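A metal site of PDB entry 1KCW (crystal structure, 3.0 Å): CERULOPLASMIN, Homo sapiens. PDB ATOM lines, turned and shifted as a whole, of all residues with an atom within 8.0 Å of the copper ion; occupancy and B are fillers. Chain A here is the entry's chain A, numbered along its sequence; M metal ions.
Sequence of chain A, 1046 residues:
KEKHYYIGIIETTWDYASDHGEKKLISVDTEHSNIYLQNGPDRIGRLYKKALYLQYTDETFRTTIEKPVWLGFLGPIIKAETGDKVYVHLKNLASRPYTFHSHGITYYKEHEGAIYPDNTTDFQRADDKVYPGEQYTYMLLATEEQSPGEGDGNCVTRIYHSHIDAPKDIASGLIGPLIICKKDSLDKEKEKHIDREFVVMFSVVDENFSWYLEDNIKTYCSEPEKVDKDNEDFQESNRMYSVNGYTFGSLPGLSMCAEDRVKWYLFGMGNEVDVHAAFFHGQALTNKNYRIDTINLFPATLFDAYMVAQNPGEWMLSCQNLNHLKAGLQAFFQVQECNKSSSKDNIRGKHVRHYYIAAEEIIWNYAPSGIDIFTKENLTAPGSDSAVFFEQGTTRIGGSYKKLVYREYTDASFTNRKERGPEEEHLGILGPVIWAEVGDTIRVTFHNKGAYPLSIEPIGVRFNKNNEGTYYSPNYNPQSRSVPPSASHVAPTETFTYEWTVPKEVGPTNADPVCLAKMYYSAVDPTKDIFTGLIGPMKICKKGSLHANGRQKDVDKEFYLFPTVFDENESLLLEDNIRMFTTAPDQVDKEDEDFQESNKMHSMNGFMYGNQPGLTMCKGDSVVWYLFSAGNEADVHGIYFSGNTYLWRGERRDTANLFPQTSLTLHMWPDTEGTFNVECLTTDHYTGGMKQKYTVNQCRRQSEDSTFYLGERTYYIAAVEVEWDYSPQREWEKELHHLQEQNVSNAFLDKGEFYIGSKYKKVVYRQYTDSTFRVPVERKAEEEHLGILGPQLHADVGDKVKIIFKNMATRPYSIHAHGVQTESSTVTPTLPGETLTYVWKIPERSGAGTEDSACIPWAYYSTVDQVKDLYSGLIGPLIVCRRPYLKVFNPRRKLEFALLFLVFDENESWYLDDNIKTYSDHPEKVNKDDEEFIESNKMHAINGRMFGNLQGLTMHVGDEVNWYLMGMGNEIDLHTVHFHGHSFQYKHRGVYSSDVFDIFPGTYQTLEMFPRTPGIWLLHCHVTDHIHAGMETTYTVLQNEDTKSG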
ATOM      1  N   PHE A 202      29.131  21.460  10.263  1.00  0.00           N
ATOM      2  CA  PHE A 202      28.796  22.757  10.833  1.00  0.00           C
ATOM      3  C   PHE A 202      28.253  22.415  12.196  1.00  0.00           C
ATOM      4  O   PHE A 202      27.563  21.404  12.327  1.00  0.00           O
ATOM      5  CB  PHE A 202      27.739  23.497  10.013  1.00  0.00           C
ATOM      6  CG  PHE A 202      28.294  24.223   8.816  1.00  0.00           C
ATOM      7  CD1 PHE A 202      28.918  23.531   7.791  1.00  0.00           C
ATOM      8  CD2 PHE A 202      28.221  25.601   8.751  1.00  0.00           C
ATOM      9  CE1 PHE A 202      29.450  24.190   6.727  1.00  0.00           C
ATOM     10  CE2 PHE A 202      28.754  26.281   7.674  1.00  0.00           C
ATOM     11  CZ  PHE A 202      29.372  25.576   6.657  1.00  0.00           C
ATOM     12  N   SER A 203      28.636  23.215  13.193  1.00  0.00           N
ATOM     13  CA  SER A 203      28.177  23.024  14.568  1.00  0.00           C
ATOM     14  C   SER A 203      28.620  24.152  15.514  1.00  0.00           C
ATOM     15  O   SER A 203      29.725  24.678  15.396  1.00  0.00           O
ATOM     16  CB  SER A 203      28.679  21.684  15.117  1.00  0.00           C
ATOM     17  OG  SER A 203      28.489  21.597  16.517  1.00  0.00           O
ATOM     18  N   VAL A 204      27.717  24.519  16.422  1.00  0.00           N
ATOM     19  CA  VAL A 204      28.030  25.431  17.522  1.00  0.00           C
ATOM     20  C   VAL A 204      28.496  24.520  18.634  1.00  0.00           C
ATOM     21  O   VAL A 204      27.736  24.270  19.586  1.00  0.00           O
ATOM     22  CB  VAL A 204      26.748  26.169  17.980  1.00  0.00           C
ATOM     23  CG1 VAL A 204      27.058  27.124  19.113  1.00  0.00           C
ATOM     24  CG2 VAL A 204      26.088  26.879  16.812  1.00  0.00           C
ATOM     25  N   TYR A 241      31.073  28.534  17.623  1.00  0.00           N
ATOM     26  CA  TYR A 241      30.522  28.490  16.269  1.00  0.00           C
ATOM     27  C   TYR A 241      31.630  28.102  15.318  1.00  0.00           C
ATOM     28  O   TYR A 241      32.510  28.908  15.049  1.00  0.00           O
ATOM     29  CB  TYR A 241      29.942  29.866  15.943  1.00  0.00           C
ATOM     30  CG  TYR A 241      28.832  30.318  16.890  1.00  0.00           C
ATOM     31  CD1 TYR A 241      29.103  30.732  18.182  1.00  0.00           C
ATOM     32  CD2 TYR A 241      27.499  30.315  16.481  1.00  0.00           C
ATOM     33  CE1 TYR A 241      28.063  31.143  19.033  1.00  0.00           C
ATOM     34  CE2 TYR A 241      26.475  30.710  17.331  1.00  0.00           C
ATOM     35  CZ  TYR A 241      26.756  31.117  18.595  1.00  0.00           C
ATOM     36  OH  TYR A 241      25.718  31.498  19.413  1.00  0.00           O
ATOM     37  N   SER A 242      31.589  26.905  14.747  1.00  0.00           N
ATOM     38  CA  SER A 242      32.699  26.477  13.919  1.00  0.00           C
ATOM     39  C   SER A 242      32.421  25.494  12.965  1.00  0.00           C
ATOM     40  O   SER A 242      31.638  24.590  13.196  1.00  0.00           O
ATOM     41  CB  SER A 242      33.752  25.967  14.867  1.00  0.00           C
ATOM     42  OG  SER A 242      33.231  24.956  15.719  1.00  0.00           O
ATOM     43  N   VAL A 273      19.763  25.632  18.309  1.00  0.00           N
ATOM     44  CA  VAL A 273      20.198  26.930  17.827  1.00  0.00           C
ATOM     45  C   VAL A 273      21.092  26.560  16.674  1.00  0.00           C
ATOM     46  O   VAL A 273      21.874  27.376  16.233  1.00  0.00           O
ATOM     47  CB  VAL A 273      21.002  27.755  18.896  1.00  0.00           C
ATOM     48  CG1 VAL A 273      20.227  27.830  20.191  1.00  0.00           C
ATOM     49  CG2 VAL A 273      22.379  27.164  19.127  1.00  0.00           C
ATOM     50  N   ASP A 274      20.977  25.327  16.213  1.00  0.00           N
ATOM     51  CA  ASP A 274      21.829  24.889  15.120  1.00  0.00           C
ATOM     52  C   ASP A 274      21.136  24.889  13.767  1.00  0.00           C
ATOM     53  O   ASP A 274      21.039  23.871  13.077  1.00  0.00           O
ATOM     54  CB  ASP A 274      22.438  23.538  15.428  1.00  0.00           C
ATOM     55  CG  ASP A 274      23.693  23.658  16.234  1.00  0.00           C
ATOM     56  OD1 ASP A 274      23.631  23.667  17.486  1.00  0.00           O
ATOM     57  OD2 ASP A 274      24.749  23.747  15.605  1.00  0.00           O
ATOM     58  N   VAL A 275      20.677  26.087  13.398  1.00  0.00           N
ATOM     59  CA  VAL A 275      20.001  26.294  12.152  1.00  0.00           C
ATOM     60  C   VAL A 275      21.101  26.871  11.261  1.00  0.00           C
ATOM     61  O   VAL A 275      21.443  28.042  11.373  1.00  0.00           O
ATOM     62  CB  VAL A 275      18.890  27.294  12.384  1.00  0.00           C
ATOM     63  CG1 VAL A 275      18.215  27.641  11.095  1.00  0.00           C
ATOM     64  CG2 VAL A 275      17.903  26.725  13.360  1.00  0.00           C
ATOM     65  N   HIS A 276      21.710  26.013  10.452  1.00  0.00           N
ATOM     66  CA  HIS A 276      22.791  26.444   9.592  1.00  0.00           C
ATOM     67  C   HIS A 276      22.388  26.673   8.165  1.00  0.00           C
ATOM     68  O   HIS A 276      21.375  26.168   7.720  1.00  0.00           O
ATOM     69  CB  HIS A 276      23.950  25.431   9.620  1.00  0.00           C
ATOM     70  CG  HIS A 276      24.496  25.199  10.998  1.00  0.00           C
ATOM     71  ND1 HIS A 276      25.230  26.156  11.630  1.00  0.00           N
ATOM     72  CD2 HIS A 276      24.158  24.227  11.872  1.00  0.00           C
ATOM     73  CE1 HIS A 276      25.311  25.760  12.891  1.00  0.00           C
ATOM     74  NE2 HIS A 276      24.677  24.590  13.079  1.00  0.00           N
ATOM     75  N   ALA A 277      23.258  27.373   7.440  1.00  0.00           N
ATOM     76  CA  ALA A 277      23.058  27.696   6.033  1.00  0.00           C
ATOM     77  C   ALA A 277      24.428  27.730   5.398  1.00  0.00           C
ATOM     78  O   ALA A 277      25.004  28.797   5.225  1.00  0.00           O
ATOM     79  CB  ALA A 277      22.396  29.039   5.906  1.00  0.00           C
ATOM     80  N   ALA A 278      24.984  26.565   5.121  1.00  0.00           N
ATOM     81  CA  ALA A 278      26.302  26.482   4.518  1.00  0.00           C
ATOM     82  C   ALA A 278      26.277  27.171   3.170  1.00  0.00           C
ATOM     83  O   ALA A 278      25.385  26.929   2.370  1.00  0.00           O
ATOM     84  CB  ALA A 278      26.699  25.052   4.344  1.00  0.00           C
ATOM     85  N   LEU A 297      21.605  22.851   7.205  1.00  0.00           N
ATOM     86  CA  LEU A 297      22.019  21.726   8.020  1.00  0.00           C
ATOM     87  C   LEU A 297      21.541  21.955   9.418  1.00  0.00           C
ATOM     88  O   LEU A 297      21.644  23.062   9.938  1.00  0.00           O
ATOM     89  CB  LEU A 297      23.532  21.655   8.047  1.00  0.00           C
ATOM     90  CG  LEU A 297      24.142  21.398   6.666  1.00  0.00           C
ATOM     91  CD1 LEU A 297      25.676  21.375   6.729  1.00  0.00           C
ATOM     92  CD2 LEU A 297      23.620  20.089   6.121  1.00  0.00           C
ATOM     93  N   SER A 318      30.745  30.027   4.471  1.00  0.00           N
ATOM     94  CA  SER A 318      30.211  30.561   5.708  1.00  0.00           C
ATOM     95  C   SER A 318      28.835  29.984   5.974  1.00  0.00           C
ATOM     96  O   SER A 318      28.342  29.166   5.193  1.00  0.00           O
ATOM     97  CB  SER A 318      30.166  32.094   5.688  1.00  0.00           C
ATOM     98  OG  SER A 318      29.283  32.572   4.698  1.00  0.00           O
ATOM     99  N   CYS A 319      28.242  30.378   7.084  1.00  0.00           N
ATOM    100  CA  CYS A 319      26.927  29.904   7.408  1.00  0.00           C
ATOM    101  C   CYS A 319      26.037  31.156   7.401  1.00  0.00           C
ATOM    102  O   CYS A 319      26.084  31.968   8.332  1.00  0.00           O
ATOM    103  CB  CYS A 319      26.959  29.229   8.773  1.00  0.00           C
ATOM    104  SG  CYS A 319      25.392  28.961   9.495  1.00  0.00           S
ATOM    105  N   GLN A 320      25.254  31.315   6.338  1.00  0.00           N
ATOM    106  CA  GLN A 320      24.395  32.477   6.176  1.00  0.00           C
ATOM    107  C   GLN A 320      23.430  32.752   7.299  1.00  0.00           C
ATOM    108  O   GLN A 320      22.698  33.753   7.266  1.00  0.00           O
ATOM    109  CB  GLN A 320      23.677  32.429   4.844  1.00  0.00           C
ATOM    110  CG  GLN A 320      24.576  32.625   3.651  1.00  0.00           C
ATOM    111  CD  GLN A 320      25.628  33.670   3.937  1.00  0.00           C
ATOM    112  OE1 GLN A 320      25.299  34.774   4.366  1.00  0.00           O
ATOM    113  NE2 GLN A 320      26.927  33.531   3.756  1.00  0.00           N
ATOM    114  N   ASN A 321      23.352  31.901   8.290  1.00  0.00           N
ATOM    115  CA  ASN A 321      22.574  32.279   9.447  1.00  0.00           C
ATOM    116  C   ASN A 321      23.276  33.519   9.970  1.00  0.00           C
ATOM    117  O   ASN A 321      24.458  33.459  10.295  1.00  0.00           O
ATOM    118  CB  ASN A 321      22.537  31.142  10.456  1.00  0.00           C
ATOM    119  CG  ASN A 321      21.935  31.561  11.774  1.00  0.00           C
ATOM    120  OD1 ASN A 321      21.927  32.736  12.122  1.00  0.00           O
ATOM    121  ND2 ASN A 321      21.418  30.584  12.507  1.00  0.00           N
ATOM    122  N   LEU A 322      22.584  34.654  10.027  1.00  0.00           N
ATOM    123  CA  LEU A 322      23.231  35.882  10.479  1.00  0.00           C
ATOM    124  C   LEU A 322      23.917  35.797  11.809  1.00  0.00           C
ATOM    125  O   LEU A 322      25.112  36.072  11.883  1.00  0.00           O
ATOM    126  CB  LEU A 322      22.274  37.075  10.478  1.00  0.00           C
ATOM    127  CG  LEU A 322      21.670  37.388   9.105  1.00  0.00           C
ATOM    128  CD1 LEU A 322      20.699  38.527   9.302  1.00  0.00           C
ATOM    129  CD2 LEU A 322      22.712  37.703   8.012  1.00  0.00           C
ATOM    130  N   ASN A 323      23.201  35.369  12.848  1.00  0.00           N
ATOM    131  CA  ASN A 323      23.840  35.265  14.159  1.00  0.00           C
ATOM    132  C   ASN A 323      25.102  34.408  14.186  1.00  0.00           C
ATOM    133  O   ASN A 323      26.065  34.729  14.884  1.00  0.00           O
ATOM    134  CB  ASN A 323      22.839  34.811  15.192  1.00  0.00           C
ATOM    135  CG  ASN A 323      21.925  35.915  15.596  1.00  0.00           C
ATOM    136  OD1 ASN A 323      21.900  36.976  14.957  1.00  0.00           O
ATOM    137  ND2 ASN A 323      21.178  35.716  16.674  1.00  0.00           N
ATOM    138  N   HIS A 324      25.132  33.360  13.390  1.00  0.00           N
ATOM    139  CA  HIS A 324      26.281  32.502  13.343  1.00  0.00           C
ATOM    140  C   HIS A 324      27.378  33.224  12.597  1.00  0.00           C
ATOM    141  O   HIS A 324      28.526  33.216  13.016  1.00  0.00           O
ATOM    142  CB  HIS A 324      25.916  31.147  12.699  1.00  0.00           C
ATOM    143  CG  HIS A 324      24.977  30.318  13.531  1.00  0.00           C
ATOM    144  ND1 HIS A 324      24.535  29.091  13.129  1.00  0.00           N
ATOM    145  CD2 HIS A 324      24.325  30.673  14.675  1.00  0.00           C
ATOM    146  CE1 HIS A 324      23.632  28.714  13.994  1.00  0.00           C
ATOM    147  NE2 HIS A 324      23.461  29.654  14.955  1.00  0.00           N
ATOM    148  N   LEU A 325      27.012  33.945  11.550  1.00  0.00           N
ATOM    149  CA  LEU A 325      27.999  34.687  10.767  1.00  0.00           C
ATOM    150  C   LEU A 325      28.790  35.701  11.625  1.00  0.00           C
ATOM    151  O   LEU A 325      30.007  35.801  11.497  1.00  0.00           O
ATOM    152  CB  LEU A 325      27.300  35.414   9.633  1.00  0.00           C
ATOM    153  CG  LEU A 325      28.224  36.164   8.677  1.00  0.00           C
ATOM    154  CD1 LEU A 325      28.667  35.226   7.547  1.00  0.00           C
ATOM    155  CD2 LEU A 325      27.468  37.349   8.089  1.00  0.00           C
ATOM    156  N   LEU A 329      31.608  32.190  12.044  1.00  0.00           N
ATOM    157  CA  LEU A 329      31.559  30.846  11.512  1.00  0.00           C
ATOM    158  C   LEU A 329      31.959  30.968  10.067  1.00  0.00           C
ATOM    159  O   LEU A 329      31.156  30.727   9.170  1.00  0.00           O
ATOM    160  CB  LEU A 329      30.142  30.254  11.609  1.00  0.00           C
ATOM    161  CG  LEU A 329      30.065  28.707  11.645  1.00  0.00           C
ATOM    162  CD1 LEU A 329      28.763  28.294  12.262  1.00  0.00           C
ATOM    163  CD2 LEU A 329      30.258  28.058  10.287  1.00  0.00           C
ATOM    164  N   GLU A 633      18.369  32.188  13.397  1.00  0.00           N
ATOM    165  CA  GLU A 633      17.862  30.856  13.690  1.00  0.00           C
ATOM    166  C   GLU A 633      16.391  30.839  14.042  1.00  0.00           C
ATOM    167  O   GLU A 633      15.828  29.787  14.377  1.00  0.00           O
ATOM    168  CB  GLU A 633      18.685  30.192  14.794  1.00  0.00           C
ATOM    169  CG  GLU A 633      18.509  30.806  16.189  1.00  0.00           C
ATOM    170  CD  GLU A 633      19.584  31.822  16.539  1.00  0.00           C
ATOM    171  OE1 GLU A 633      20.648  31.881  15.869  1.00  0.00           O
ATOM    172  OE2 GLU A 633      19.356  32.567  17.521  1.00  0.00           O
ATOM    173  N   PRO A 660      17.134  30.321   6.977  1.00  0.00           N
ATOM    174  CA  PRO A 660      18.060  31.333   6.474  1.00  0.00           C
ATOM    175  C   PRO A 660      18.640  31.063   5.086  1.00  0.00           C
ATOM    176  O   PRO A 660      19.404  30.121   4.909  1.00  0.00           O
ATOM    177  CB  PRO A 660      19.142  31.326   7.533  1.00  0.00           C
ATOM    178  CG  PRO A 660      18.322  31.155   8.788  1.00  0.00           C
ATOM    179  CD  PRO A 660      17.417  30.021   8.389  1.00  0.00           C
HETATM  180 CU    CU M   1      25.154  28.239  11.367  1.00  0.00          CU
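The copper ion is bound by the side-chain sulfur (SG) of Cys 319 (2.0 Å), a ring nitrogen (ND1) of His 324 (2.1 Å) and a ring nitrogen (ND1) of His 276 (2.1 Å).
The copper ion has three donor atoms within binding distance.
Merely in contact with the copper ion: Val 275 (3.7 Å) and Leu 329 (3.7 Å).
Within 4 Å of the copper ion: Val 275, His 276, Cys 319, His 324 and Leu 329.
The nearest printed residue that does not touch the copper ion is Asn 321 (4.01 Å).
A ring nitrogen (NE2) of His 276 lies within hydrogen-bond range of the side-chain carboxylate (OD2) of Asp 274 (2.7 Å).
SG of Cys 319 lies close to N of Asn 321, at 3.8 Å.
A ring nitrogen (NE2) of His 324 sits at hydrogen-bond distance from the backbone carbonyl oxygen (O) of Val 273 (3.1 Å).
The side-chain amide nitrogen (ND2) of Asn 321 lies close to a ring nitrogen (NE2) of His 324 (3.3 Å).
The backbone NH (N) of Leu 329 sits at hydrogen-bond distance from the backbone carbonyl oxygen (O) of His 324 (3.4 Å).
The backbone NH (N) of His 276 lies within hydrogen-bond range of the backbone carbonyl oxygen (O) of Leu 297 (3.0 Å).
O of Val 275 is in hydrogen-bond range of ND2 of Asn 321, 2.8 Å away.
N of Ala 277 sits close to SG of Cys 319 (3.4 Å).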
